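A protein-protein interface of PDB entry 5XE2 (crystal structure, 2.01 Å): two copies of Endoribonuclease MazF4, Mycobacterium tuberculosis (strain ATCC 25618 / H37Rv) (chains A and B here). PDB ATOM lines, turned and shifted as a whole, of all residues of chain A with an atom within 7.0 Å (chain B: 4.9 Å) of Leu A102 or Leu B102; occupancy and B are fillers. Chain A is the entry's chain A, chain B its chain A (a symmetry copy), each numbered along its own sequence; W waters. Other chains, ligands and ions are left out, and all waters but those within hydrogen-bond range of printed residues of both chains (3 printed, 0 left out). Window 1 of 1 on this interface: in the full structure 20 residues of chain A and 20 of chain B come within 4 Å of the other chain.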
ATOM      1  N   ARG A   8      22.952  -9.428  -9.371  1.00  0.00           N
ATOM      2  CA  ARG A   8      22.903  -9.811 -10.776  1.00  0.00           C
ATOM      3  C   ARG A   8      22.040  -8.799 -11.535  1.00  0.00           C
ATOM      4  O   ARG A   8      20.996  -8.370 -11.032  1.00  0.00           O
ATOM      5  CB  ARG A   8      22.341 -11.219 -10.923  1.00  0.00           C
ATOM      6  CG  ARG A   8      22.619 -11.847 -12.269  1.00  0.00           C
ATOM      7  CD  ARG A   8      22.351 -13.339 -12.265  1.00  0.00           C
ATOM      8  NE  ARG A   8      22.830 -13.945 -13.502  1.00  0.00           N
ATOM      9  CZ  ARG A   8      22.189 -13.947 -14.674  1.00  0.00           C
ATOM     10  NH1 ARG A   8      20.994 -13.370 -14.823  1.00  0.00           N
ATOM     11  NH2 ARG A   8      22.759 -14.540 -15.721  1.00  0.00           N
ATOM     12  N   VAL A  26      27.007 -10.767 -13.634  1.00  0.00           N
ATOM     13  CA  VAL A  26      26.302 -11.986 -14.084  1.00  0.00           C
ATOM     14  C   VAL A  26      26.378 -13.183 -13.126  1.00  0.00           C
ATOM     15  O   VAL A  26      25.658 -14.169 -13.315  1.00  0.00           O
ATOM     16  CB  VAL A  26      26.720 -12.392 -15.518  1.00  0.00           C
ATOM     17  CG1 VAL A  26      26.282 -11.308 -16.504  1.00  0.00           C
ATOM     18  CG2 VAL A  26      28.224 -12.628 -15.630  1.00  0.00           C
ATOM     19  N   SER A  27      27.209 -13.098 -12.092  1.00  0.00           N
ATOM     20  CA  SER A  27      27.249 -14.132 -11.063  1.00  0.00           C
ATOM     21  C   SER A  27      25.966 -14.129 -10.218  1.00  0.00           C
ATOM     22  O   SER A  27      25.283 -13.113 -10.102  1.00  0.00           O
ATOM     23  CB  SER A  27      28.498 -13.988 -10.181  1.00  0.00           C
ATOM     24  OG  SER A  27      28.846 -12.630  -9.981  1.00  0.00           O
ATOM     25  N   ASN A  28      25.646 -15.289  -9.653  1.00  0.00           N
ATOM     26  CA  ASN A  28      24.443 -15.450  -8.846  1.00  0.00           C
ATOM     27  C   ASN A  28      24.524 -14.654  -7.540  1.00  0.00           C
ATOM     28  O   ASN A  28      25.618 -14.436  -6.991  1.00  0.00           O
ATOM     29  CB  ASN A  28      24.159 -16.939  -8.582  1.00  0.00           C
ATOM     30  CG  ASN A  28      25.109 -17.558  -7.561  1.00  0.00           C
ATOM     31  OD1 ASN A  28      25.041 -17.253  -6.368  1.00  0.00           O
ATOM     32  ND2 ASN A  28      25.983 -18.440  -8.017  1.00  0.00           N
ATOM     33  N   ARG A  31      26.511 -16.008  -4.261  1.00  0.00           N
ATOM     34  CA  ARG A  31      27.953 -15.794  -4.426  1.00  0.00           C
ATOM     35  C   ARG A  31      28.296 -14.311  -4.279  1.00  0.00           C
ATOM     36  O   ARG A  31      29.287 -13.965  -3.616  1.00  0.00           O
ATOM     37  CB  ARG A  31      28.439 -16.340  -5.781  1.00  0.00           C
ATOM     38  CG  ARG A  31      29.938 -16.187  -6.066  1.00  0.00           C
ATOM     39  CD  ARG A  31      30.273 -14.875  -6.777  1.00  0.00           C
ATOM     40  NE  ARG A  31      31.681 -14.754  -7.151  1.00  0.00           N
ATOM     41  CZ  ARG A  31      32.251 -15.322  -8.219  1.00  0.00           C
ATOM     42  NH1 ARG A  31      31.552 -16.087  -9.064  1.00  0.00           N
ATOM     43  NH2 ARG A  31      33.556 -15.124  -8.448  1.00  0.00           N
ATOM     44  N   VAL A  39      31.464 -12.125 -10.864  1.00  0.00           N
ATOM     45  CA  VAL A  39      31.735 -12.297 -12.280  1.00  0.00           C
ATOM     46  C   VAL A  39      30.860 -11.316 -13.047  1.00  0.00           C
ATOM     47  O   VAL A  39      29.687 -11.112 -12.712  1.00  0.00           O
ATOM     48  CB  VAL A  39      31.510 -13.742 -12.750  1.00  0.00           C
ATOM     49  CG1 VAL A  39      31.704 -13.864 -14.253  1.00  0.00           C
ATOM     50  CG2 VAL A  39      32.468 -14.671 -12.028  1.00  0.00           C
ATOM     51  N   ALA A  40      31.470 -10.701 -14.060  1.00  0.00           N
ATOM     52  CA  ALA A  40      30.832  -9.677 -14.855  1.00  0.00           C
ATOM     53  C   ALA A  40      31.220  -9.772 -16.329  1.00  0.00           C
ATOM     54  O   ALA A  40      32.238 -10.381 -16.694  1.00  0.00           O
ATOM     55  CB  ALA A  40      31.201  -8.307 -14.303  1.00  0.00           C
ATOM     56  N   VAL A  41      30.385  -9.154 -17.162  1.00  0.00           N
ATOM     57  CA  VAL A  41      30.637  -9.008 -18.591  1.00  0.00           C
ATOM     58  C   VAL A  41      30.666  -7.533 -18.978  1.00  0.00           C
ATOM     59  O   VAL A  41      30.001  -6.677 -18.355  1.00  0.00           O
ATOM     60  CB  VAL A  41      29.601  -9.743 -19.468  1.00  0.00           C
ATOM     61  CG1 VAL A  41      29.769 -11.252 -19.335  1.00  0.00           C
ATOM     62  CG2 VAL A  41      28.174  -9.311 -19.148  1.00  0.00           C
ATOM     63  N   THR A  52      26.514 -13.470 -29.371  1.00  0.00           N
ATOM     64  CA  THR A  52      27.045 -13.184 -28.022  1.00  0.00           C
ATOM     65  C   THR A  52      27.045 -11.705 -27.607  1.00  0.00           C
ATOM     66  O   THR A  52      27.497 -11.378 -26.507  1.00  0.00           O
ATOM     67  CB  THR A  52      28.457 -13.762 -27.866  1.00  0.00           C
ATOM     68  OG1 THR A  52      29.256 -13.380 -28.999  1.00  0.00           O
ATOM     69  CG2 THR A  52      28.378 -15.279 -27.761  1.00  0.00           C
ATOM     70  N   ALA A  68      29.069 -10.544 -24.108  1.00  0.00           N
ATOM     71  CA  ALA A  68      29.040 -11.756 -23.266  1.00  0.00           C
ATOM     72  C   ALA A  68      30.222 -12.693 -23.494  1.00  0.00           C
ATOM     73  O   ALA A  68      30.406 -13.630 -22.718  1.00  0.00           O
ATOM     74  CB  ALA A  68      27.731 -12.514 -23.455  1.00  0.00           C
ATOM     75  N   ASP A  69      31.012 -12.464 -24.548  1.00  0.00           N
ATOM     76  CA  ASP A  69      32.284 -13.183 -24.725  1.00  0.00           C
ATOM     77  C   ASP A  69      33.365 -12.763 -23.730  1.00  0.00           C
ATOM     78  O   ASP A  69      34.273 -13.545 -23.455  1.00  0.00           O
ATOM     79  CB  ASP A  69      32.824 -13.037 -26.161  1.00  0.00           C
ATOM     80  CG  ASP A  69      32.021 -13.831 -27.177  1.00  0.00           C
ATOM     81  OD1 ASP A  69      31.537 -14.928 -26.836  1.00  0.00           O
ATOM     82  OD2 ASP A  69      31.877 -13.369 -28.323  1.00  0.00           O
ATOM     83  N   ILE A  71      34.050 -12.293 -20.278  1.00  0.00           N
ATOM     84  CA  ILE A  71      33.622 -12.631 -18.930  1.00  0.00           C
ATOM     85  C   ILE A  71      34.843 -12.550 -18.015  1.00  0.00           C
ATOM     86  O   ILE A  71      35.878 -13.160 -18.301  1.00  0.00           O
ATOM     87  CB  ILE A  71      32.990 -14.045 -18.876  1.00  0.00           C
ATOM     88  CG1 ILE A  71      31.805 -14.171 -19.848  1.00  0.00           C
ATOM     89  CG2 ILE A  71      32.493 -14.367 -17.470  1.00  0.00           C
ATOM     90  CD1 ILE A  71      31.527 -15.590 -20.312  1.00  0.00           C
ATOM     91  N   MET A  91      18.059  -9.018 -19.569  1.00  0.00           N
ATOM     92  CA  MET A  91      18.824 -10.067 -18.860  1.00  0.00           C
ATOM     93  C   MET A  91      18.598 -11.466 -19.431  1.00  0.00           C
ATOM     94  O   MET A  91      19.535 -12.270 -19.469  1.00  0.00           O
ATOM     95  CB  MET A  91      18.528 -10.084 -17.351  1.00  0.00           C
ATOM     96  CG  MET A  91      19.248  -9.025 -16.531  1.00  0.00           C
ATOM     97  SD  MET A  91      21.042  -8.925 -16.778  1.00  0.00           S
ATOM     98  CE  MET A  91      21.607 -10.542 -16.282  1.00  0.00           C
ATOM     99  N   ASN A  95      21.292 -14.039 -20.667  1.00  0.00           N
ATOM    100  CA  ASN A  95      21.426 -15.452 -20.272  1.00  0.00           C
ATOM    101  C   ASN A  95      21.730 -16.360 -21.453  1.00  0.00           C
ATOM    102  O   ASN A  95      22.576 -17.245 -21.355  1.00  0.00           O
ATOM    103  CB  ASN A  95      20.174 -15.974 -19.577  1.00  0.00           C
ATOM    104  CG  ASN A  95      19.888 -15.274 -18.267  1.00  0.00           C
ATOM    105  OD1 ASN A  95      20.782 -14.709 -17.621  1.00  0.00           O
ATOM    106  ND2 ASN A  95      18.633 -15.317 -17.859  1.00  0.00           N
ATOM    107  N   THR A  96      21.033 -16.136 -22.563  1.00  0.00           N
ATOM    108  CA  THR A  96      21.226 -16.941 -23.772  1.00  0.00           C
ATOM    109  C   THR A  96      22.607 -16.681 -24.359  1.00  0.00           C
ATOM    110  O   THR A  96      23.300 -17.622 -24.747  1.00  0.00           O
ATOM    111  CB  THR A  96      20.131 -16.647 -24.818  1.00  0.00           C
ATOM    112  OG1 THR A  96      18.854 -16.867 -24.215  1.00  0.00           O
ATOM    113  CG2 THR A  96      20.273 -17.558 -26.040  1.00  0.00           C
ATOM    114  N   ALA A  97      22.991 -15.402 -24.409  1.00  0.00           N
ATOM    115  CA  ALA A  97      24.299 -14.992 -24.914  1.00  0.00           C
ATOM    116  C   ALA A  97      25.463 -15.619 -24.116  1.00  0.00           C
ATOM    117  O   ALA A  97      26.430 -16.129 -24.699  1.00  0.00           O
ATOM    118  CB  ALA A  97      24.399 -13.472 -24.910  1.00  0.00           C
ATOM    119  N   LEU A  98      25.366 -15.580 -22.788  1.00  0.00           N
ATOM    120  CA  LEU A  98      26.340 -16.244 -21.915  1.00  0.00           C
ATOM    121  C   LEU A  98      26.436 -17.753 -22.171  1.00  0.00           C
ATOM    122  O   LEU A  98      27.537 -18.302 -22.260  1.00  0.00           O
ATOM    123  CB  LEU A  98      25.991 -16.000 -20.449  1.00  0.00           C
ATOM    124  CG  LEU A  98      26.177 -14.596 -19.880  1.00  0.00           C
ATOM    125  CD1 LEU A  98      25.496 -14.499 -18.530  1.00  0.00           C
ATOM    126  CD2 LEU A  98      27.657 -14.250 -19.756  1.00  0.00           C
ATOM    127  N   ALA A  99      25.286 -18.424 -22.289  1.00  0.00           N
ATOM    128  CA  ALA A  99      25.260 -19.856 -22.627  1.00  0.00           C
ATOM    129  C   ALA A  99      25.964 -20.146 -23.963  1.00  0.00           C
ATOM    130  O   ALA A  99      26.728 -21.103 -24.075  1.00  0.00           O
ATOM    131  CB  ALA A  99      23.822 -20.375 -22.653  1.00  0.00           C
ATOM    132  N   THR A 100      25.724 -19.301 -24.963  1.00  0.00           N
ATOM    133  CA  THR A 100      26.382 -19.440 -26.265  1.00  0.00           C
ATOM    134  C   THR A 100      27.888 -19.196 -26.177  1.00  0.00           C
ATOM    135  O   THR A 100      28.682 -19.961 -26.745  1.00  0.00           O
ATOM    136  CB  THR A 100      25.738 -18.517 -27.317  1.00  0.00           C
ATOM    137  OG1 THR A 100      24.353 -18.843 -27.420  1.00  0.00           O
ATOM    138  CG2 THR A 100      26.381 -18.701 -28.683  1.00  0.00           C
ATOM    139  N   ALA A 101      28.285 -18.153 -25.445  1.00  0.00           N
ATOM    140  CA  ALA A 101      29.699 -17.841 -25.277  1.00  0.00           C
ATOM    141  C   ALA A 101      30.468 -19.022 -24.651  1.00  0.00           C
ATOM    142  O   ALA A 101      31.567 -19.329 -25.077  1.00  0.00           O
ATOM    143  CB  ALA A 101      29.866 -16.587 -24.443  1.00  0.00           C
ATOM    144  N   LEU A 102      29.846 -19.699 -23.684  1.00  0.00           N
ATOM    145  CA  LEU A 102      30.466 -20.797 -22.936  1.00  0.00           C
ATOM    146  C   LEU A 102      30.121 -22.213 -23.431  1.00  0.00           C
ATOM    147  O   LEU A 102      30.331 -23.187 -22.700  1.00  0.00           O
ATOM    148  CB  LEU A 102      30.076 -20.664 -21.463  1.00  0.00           C
ATOM    149  CG  LEU A 102      30.572 -19.376 -20.799  1.00  0.00           C
ATOM    150  CD1 LEU A 102      29.757 -19.057 -19.563  1.00  0.00           C
ATOM    151  CD2 LEU A 102      32.035 -19.500 -20.444  1.00  0.00           C
ATOM    152  N   GLY A 103      29.597 -22.325 -24.653  1.00  0.00           N
ATOM    153  CA  GLY A 103      29.327 -23.614 -25.290  1.00  0.00           C
ATOM    154  C   GLY A 103      28.426 -24.546 -24.507  1.00  0.00           C
ATOM    155  O   GLY A 103      28.607 -25.759 -24.560  1.00  0.00           O
ATOM    156  N   LEU A 104      27.452 -23.991 -23.789  1.00  0.00           N
ATOM    157  CA  LEU A 104      26.551 -24.802 -22.977  1.00  0.00           C
ATOM    158  C   LEU A 104      25.442 -25.353 -23.868  1.00  0.00           C
ATOM    159  O   LEU A 104      25.097 -24.726 -24.874  1.00  0.00           O
ATOM    160  CB  LEU A 104      25.953 -23.980 -21.837  1.00  0.00           C
ATOM    161  CG  LEU A 104      26.966 -23.251 -20.929  1.00  0.00           C
ATOM    162  CD1 LEU A 104      26.239 -22.464 -19.858  1.00  0.00           C
ATOM    163  CD2 LEU A 104      27.941 -24.221 -20.288  1.00  0.00           C
ATOM    164  N   PRO A 105      24.866 -26.519 -23.502  1.00  0.00           N
ATOM    165  CA  PRO A 105      23.820 -27.113 -24.340  1.00  0.00           C
ATOM    166  C   PRO A 105      22.424 -26.575 -24.030  1.00  0.00           C
ATOM    167  O   PRO A 105      21.458 -27.325 -24.090  1.00  0.00           O
ATOM    168  CB  PRO A 105      23.939 -28.605 -24.009  1.00  0.00           C
ATOM    169  CG  PRO A 105      24.345 -28.616 -22.578  1.00  0.00           C
ATOM    170  CD  PRO A 105      25.210 -27.398 -22.368  1.00  0.00           C
ATOM    171  N   ARG B   8      37.795 -26.136 -26.278  1.00  0.00           N
ATOM    172  CA  ARG B   8      37.011 -26.301 -25.061  1.00  0.00           C
ATOM    173  C   ARG B   8      37.382 -27.639 -24.413  1.00  0.00           C
ATOM    174  O   ARG B   8      37.555 -28.642 -25.113  1.00  0.00           O
ATOM    175  CB  ARG B   8      35.522 -26.249 -25.376  1.00  0.00           C
ATOM    176  CG  ARG B   8      34.653 -26.011 -24.164  1.00  0.00           C
ATOM    177  CD  ARG B   8      33.235 -25.631 -24.548  1.00  0.00           C
ATOM    178  NE  ARG B   8      32.487 -25.203 -23.371  1.00  0.00           N
ATOM    179  CZ  ARG B   8      31.909 -26.006 -22.474  1.00  0.00           C
ATOM    180  NH1 ARG B   8      31.964 -27.336 -22.583  1.00  0.00           N
ATOM    181  NH2 ARG B   8      31.262 -25.464 -21.445  1.00  0.00           N
ATOM    182  N   VAL B  26      36.713 -22.834 -21.345  1.00  0.00           N
ATOM    183  CA  VAL B  26      35.250 -23.046 -21.384  1.00  0.00           C
ATOM    184  C   VAL B  26      34.503 -22.291 -22.493  1.00  0.00           C
ATOM    185  O   VAL B  26      33.322 -22.560 -22.733  1.00  0.00           O
ATOM    186  CB  VAL B  26      34.599 -22.793 -20.003  1.00  0.00           C
ATOM    187  CG1 VAL B  26      35.111 -23.829 -19.000  1.00  0.00           C
ATOM    188  CG2 VAL B  26      34.874 -21.383 -19.489  1.00  0.00           C
ATOM    189  N   SER B  27      35.179 -21.381 -23.187  1.00  0.00           N
ATOM    190  CA  SER B  27      34.587 -20.712 -24.341  1.00  0.00           C
ATOM    191  C   SER B  27      34.403 -21.683 -25.517  1.00  0.00           C
ATOM    192  O   SER B  27      35.106 -22.687 -25.629  1.00  0.00           O
ATOM    193  CB  SER B  27      35.414 -19.486 -24.755  1.00  0.00           C
ATOM    194  OG  SER B  27      36.800 -19.699 -24.563  1.00  0.00           O
ATOM    195  N   ASN B  28      33.434 -21.375 -26.372  1.00  0.00           N
ATOM    196  CA  ASN B  28      33.120 -22.215 -27.522  1.00  0.00           C
ATOM    197  C   ASN B  28      34.251 -22.211 -28.554  1.00  0.00           C
ATOM    198  O   ASN B  28      34.989 -21.219 -28.690  1.00  0.00           O
ATOM    199  CB  ASN B  28      31.780 -21.798 -28.151  1.00  0.00           C
ATOM    200  CG  ASN B  28      31.868 -20.494 -28.939  1.00  0.00           C
ATOM    201  OD1 ASN B  28      32.478 -20.442 -30.010  1.00  0.00           O
ATOM    202  ND2 ASN B  28      31.248 -19.445 -28.425  1.00  0.00           N
ATOM    203  N   VAL B  39      37.885 -17.759 -22.845  1.00  0.00           N
ATOM    204  CA  VAL B  39      37.397 -17.731 -21.479  1.00  0.00           C
ATOM    205  C   VAL B  39      37.733 -19.067 -20.833  1.00  0.00           C
ATOM    206  O   VAL B  39      37.611 -20.127 -21.460  1.00  0.00           O
ATOM    207  CB  VAL B  39      35.893 -17.427 -21.399  1.00  0.00           C
ATOM    208  CG1 VAL B  39      35.395 -17.505 -19.964  1.00  0.00           C
ATOM    209  CG2 VAL B  39      35.617 -16.047 -21.966  1.00  0.00           C
ATOM    210  N   ILE B  71      35.773 -17.278 -13.324  1.00  0.00           N
ATOM    211  CA  ILE B  71      35.734 -17.249 -14.778  1.00  0.00           C
ATOM    212  C   ILE B  71      36.505 -16.014 -15.244  1.00  0.00           C
ATOM    213  O   ILE B  71      36.234 -14.900 -14.785  1.00  0.00           O
ATOM    214  CB  ILE B  71      34.276 -17.214 -15.304  1.00  0.00           C
ATOM    215  CG1 ILE B  71      33.460 -18.409 -14.783  1.00  0.00           C
ATOM    216  CG2 ILE B  71      34.245 -17.241 -16.828  1.00  0.00           C
ATOM    217  CD1 ILE B  71      31.964 -18.162 -14.719  1.00  0.00           C
ATOM    218  N   LEU B  98      29.095 -24.134 -14.279  1.00  0.00           N
ATOM    219  CA  LEU B  98      29.106 -22.819 -14.930  1.00  0.00           C
ATOM    220  C   LEU B  98      27.721 -22.161 -14.965  1.00  0.00           C
ATOM    221  O   LEU B  98      27.587 -20.974 -14.657  1.00  0.00           O
ATOM    222  CB  LEU B  98      29.646 -22.936 -16.353  1.00  0.00           C
ATOM    223  CG  LEU B  98      31.131 -23.238 -16.544  1.00  0.00           C
ATOM    224  CD1 LEU B  98      31.391 -23.612 -17.990  1.00  0.00           C
ATOM    225  CD2 LEU B  98      31.986 -22.042 -16.142  1.00  0.00           C
ATOM    226  N   ALA B  99      26.693 -22.928 -15.338  1.00  0.00           N
ATOM    227  CA  ALA B  99      25.309 -22.427 -15.318  1.00  0.00           C
ATOM    228  C   ALA B  99      24.889 -21.949 -13.917  1.00  0.00           C
ATOM    229  O   ALA B  99      24.269 -20.897 -13.773  1.00  0.00           O
ATOM    230  CB  ALA B  99      24.344 -23.495 -15.833  1.00  0.00           C
ATOM    231  N   THR B 100      25.253 -22.712 -12.890  1.00  0.00           N
ATOM    232  CA  THR B 100      24.962 -22.331 -11.505  1.00  0.00           C
ATOM    233  C   THR B 100      25.726 -21.077 -11.081  1.00  0.00           C
ATOM    234  O   THR B 100      25.148 -20.169 -10.464  1.00  0.00           O
ATOM    235  CB  THR B 100      25.240 -23.495 -10.535  1.00  0.00           C
ATOM    236  OG1 THR B 100      24.442 -24.611 -10.924  1.00  0.00           O
ATOM    237  CG2 THR B 100      24.885 -23.122  -9.105  1.00  0.00           C
ATOM    238  N   ALA B 101      27.011 -21.009 -11.434  1.00  0.00           N
ATOM    239  CA  ALA B 101      27.828 -19.849 -11.099  1.00  0.00           C
ATOM    240  C   ALA B 101      27.234 -18.551 -11.685  1.00  0.00           C
ATOM    241  O   ALA B 101      27.211 -17.534 -11.016  1.00  0.00           O
ATOM    242  CB  ALA B 101      29.251 -20.052 -11.574  1.00  0.00           C
ATOM    243  N   LEU B 102      26.711 -18.630 -12.910  1.00  0.00           N
ATOM    244  CA  LEU B 102      26.177 -17.476 -13.639  1.00  0.00           C
ATOM    245  C   LEU B 102      24.650 -17.295 -13.566  1.00  0.00           C
ATOM    246  O   LEU B 102      24.079 -16.560 -14.378  1.00  0.00           O
ATOM    247  CB  LEU B 102      26.607 -17.582 -15.103  1.00  0.00           C
ATOM    248  CG  LEU B 102      28.124 -17.541 -15.313  1.00  0.00           C
ATOM    249  CD1 LEU B 102      28.501 -18.149 -16.648  1.00  0.00           C
ATOM    250  CD2 LEU B 102      28.626 -16.120 -15.225  1.00  0.00           C
ATOM    251  N   GLY B 103      23.999 -17.959 -12.609  1.00  0.00           N
ATOM    252  CA  GLY B 103      22.568 -17.793 -12.356  1.00  0.00           C
ATOM    253  C   GLY B 103      21.666 -18.051 -13.545  1.00  0.00           C
ATOM    254  O   GLY B 103      20.636 -17.399 -13.684  1.00  0.00           O
ATOM    255  N   LEU B 104      22.041 -19.003 -14.398  1.00  0.00           N
ATOM    256  CA  LEU B 104      21.256 -19.304 -15.590  1.00  0.00           C
ATOM    257  C   LEU B 104      20.113 -20.240 -15.207  1.00  0.00           C
ATOM    258  O   LEU B 104      20.246 -21.007 -14.250  1.00  0.00           O
ATOM    259  CB  LEU B 104      22.125 -19.947 -16.669  1.00  0.00           C
ATOM    260  CG  LEU B 104      23.397 -19.167 -17.061  1.00  0.00           C
ATOM    261  CD1 LEU B 104      24.170 -19.924 -18.122  1.00  0.00           C
ATOM    262  CD2 LEU B 104      23.067 -17.771 -17.557  1.00  0.00           C
HETATM  263  O   HOH W   1      29.073 -17.237  -9.043  1.00  0.00           O
HETATM  264  O   HOH W   2      33.072 -17.403 -26.291  1.00  0.00           O
HETATM  265  O   HOH W   3      31.125 -16.705 -29.027  1.00  0.00           O
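N of Asn A28 sits at hydrogen-bond distance from O of Ala B101, at 3.1 Å. The backbone carbonyl oxygen of Leu A102 lies within hydrogen-bond range of the guanidinium group of Arg B8 (2.8 Å). ND2 of Asn A28 sits at hydrogen-bond distance from O of Thr B100 (3.1 Å). The backbone carbonyl oxygen (O) of Val A26 sits close to the backbone carbonyl oxygen (O) of Leu B102, at 3.1 Å. The backbone carbonyl oxygen (O) of Leu A102 sits close to the backbone carbonyl oxygen (O) of Val B26. The backbone NH (N) of Asn B28 is in hydrogen-bond range of the backbone carbonyl oxygen (O) of Ala A101. The backbone carbonyl oxygen (O) of Thr A100 lies within hydrogen-bond range of the side-chain amide nitrogen (ND2) of Asn B28, at 3.1 Å. O of Leu B102 sits at hydrogen-bond distance from NH2 of Arg A8 (2.8 Å).
The side-chain amide oxygen of Asn A28 lies within hydrogen-bond range of the backbone NH of Arg A31, 2.9 Å away. O of Met A91 sits close to OD1 of Asn A95 (3.3 Å). The backbone carbonyl oxygen (O) of Val B26 sits at hydrogen-bond distance from the guanidinium group (NE) of Arg B8, 2.8 Å away. O of Ala A99 is in hydrogen-bond range of N of Leu A104 (3.0 Å). N of Val A26 sits at hydrogen-bond distance from O of Val A39. The side-chain hydroxyl (OG) of Ser A27 sits at hydrogen-bond distance from the backbone NH (N) of Val A39 (2.8 Å).
CD2 of Leu B104 touches NH2 of Arg A8, 3.7 Å away. CA of Ser A27 touches O of Ala B101, 3.4 Å away. CD2 of Leu B102 touches CG1 of Val A39 (3.9 Å). Val B39 touches Asp A69. Ile B71 touches Ile A71. OD1 of Asn A95 touches CD2 of Leu B104 (3.8 Å). CD1 of Leu B102 touches CD1 of Leu A102 (3.3 Å). Arg B8 touches Gly A103 (CZ to O, 3.9 Å). CD2 of Leu A104 touches NH2 of Arg B8, at 3.7 Å. Leu B104 touches Leu A104.
Leu A98 touches none of the printed residues of chain B. Leu A102 touches four residues of chain B. Printed residues of chain A within 4 Å of Ile B71: Ile A71. Printed residues of chain A within 4 Å of Ala B101: Ser A27 and Asn A28. Of chain A, only Arg A8, Val A26, Val A39 and Leu A102 come within 4 Å of Leu B102. Of the printed residues of chain A, Gly B103 touches Arg A8. The nearest residue of chain B that does not touch Leu A102 is Ser B27 (4.4 Å). The nearest residue of chain A that does not touch Leu B102 is Ser A27 (4.4 Å).
Printed residues of chain A that touch a printed residue of chain B: Arg A8, Val A26, Ser A27, Asn A28, Val A39, Asp A69, Ile A71, Asn A95, Thr A100, Ala A101, Leu A102, Gly A103 and Leu A104. Hydrophobic or aromatic side chains of chain A that line the printed part of chain B: Val A26, Val A39, Ile A71, Leu A102 and Leu A104. Along chain A the printed residues that touch a printed residue of chain B span positions 8 to 104. Printed residues of chain B that touch a printed residue of chain A: Arg B8, Val B26, Ser B27, Asn B28, Val B39, Ile B71, Thr B100, Ala B101, Leu B102, Gly B103 and Leu B104. Hydrophobic or aromatic side chains of chain B within 4 Å of the printed part of chain A: Val B26, Val B39, Ile B71, Leu B102 and Leu B104. Among the printed residues, 21 pairs touch across the chains. Among the printed residues, no Asp or Glu carboxylate lies within 4 Å of a Lys or Arg side-chain nitrogen of the other chain.
Arg A8 touches Leu B102, and with the chains exchanged Leu A102 touches Arg B8. Arg A8 touches Leu B104, and with the chains exchanged Leu A104 touches Arg B8. Asn A28 touches Ala B101, and with the chains exchanged Ala A101 touches Asn B28. Ile A71 touches its own counterpart, Ile B71. Positions printed for both chains: 8, 26, 27, 28, 39, 71, 98, 99, 100, 101, 102, 103 and 104.
Water W1 lies within hydrogen-bond range of the backbone carbonyl oxygen (O) of Ala B101 (2.7 Å), the guanidinium group (NH1) of Arg A31 (2.7 Å) and the side-chain amide nitrogen (ND2) of Asn A28 (3.5 Å). Water W2 lies within hydrogen-bond range of the backbone carbonyl oxygen of Ala A101, the side-chain carboxylate of Asp A69 and the side-chain amide nitrogen of Asn B28. Water W3 lies within hydrogen-bond range of the side-chain amide nitrogen of Asn B28 (2.8 Å) and the side-chain carboxylate of Asp A69 (2.9 Å).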
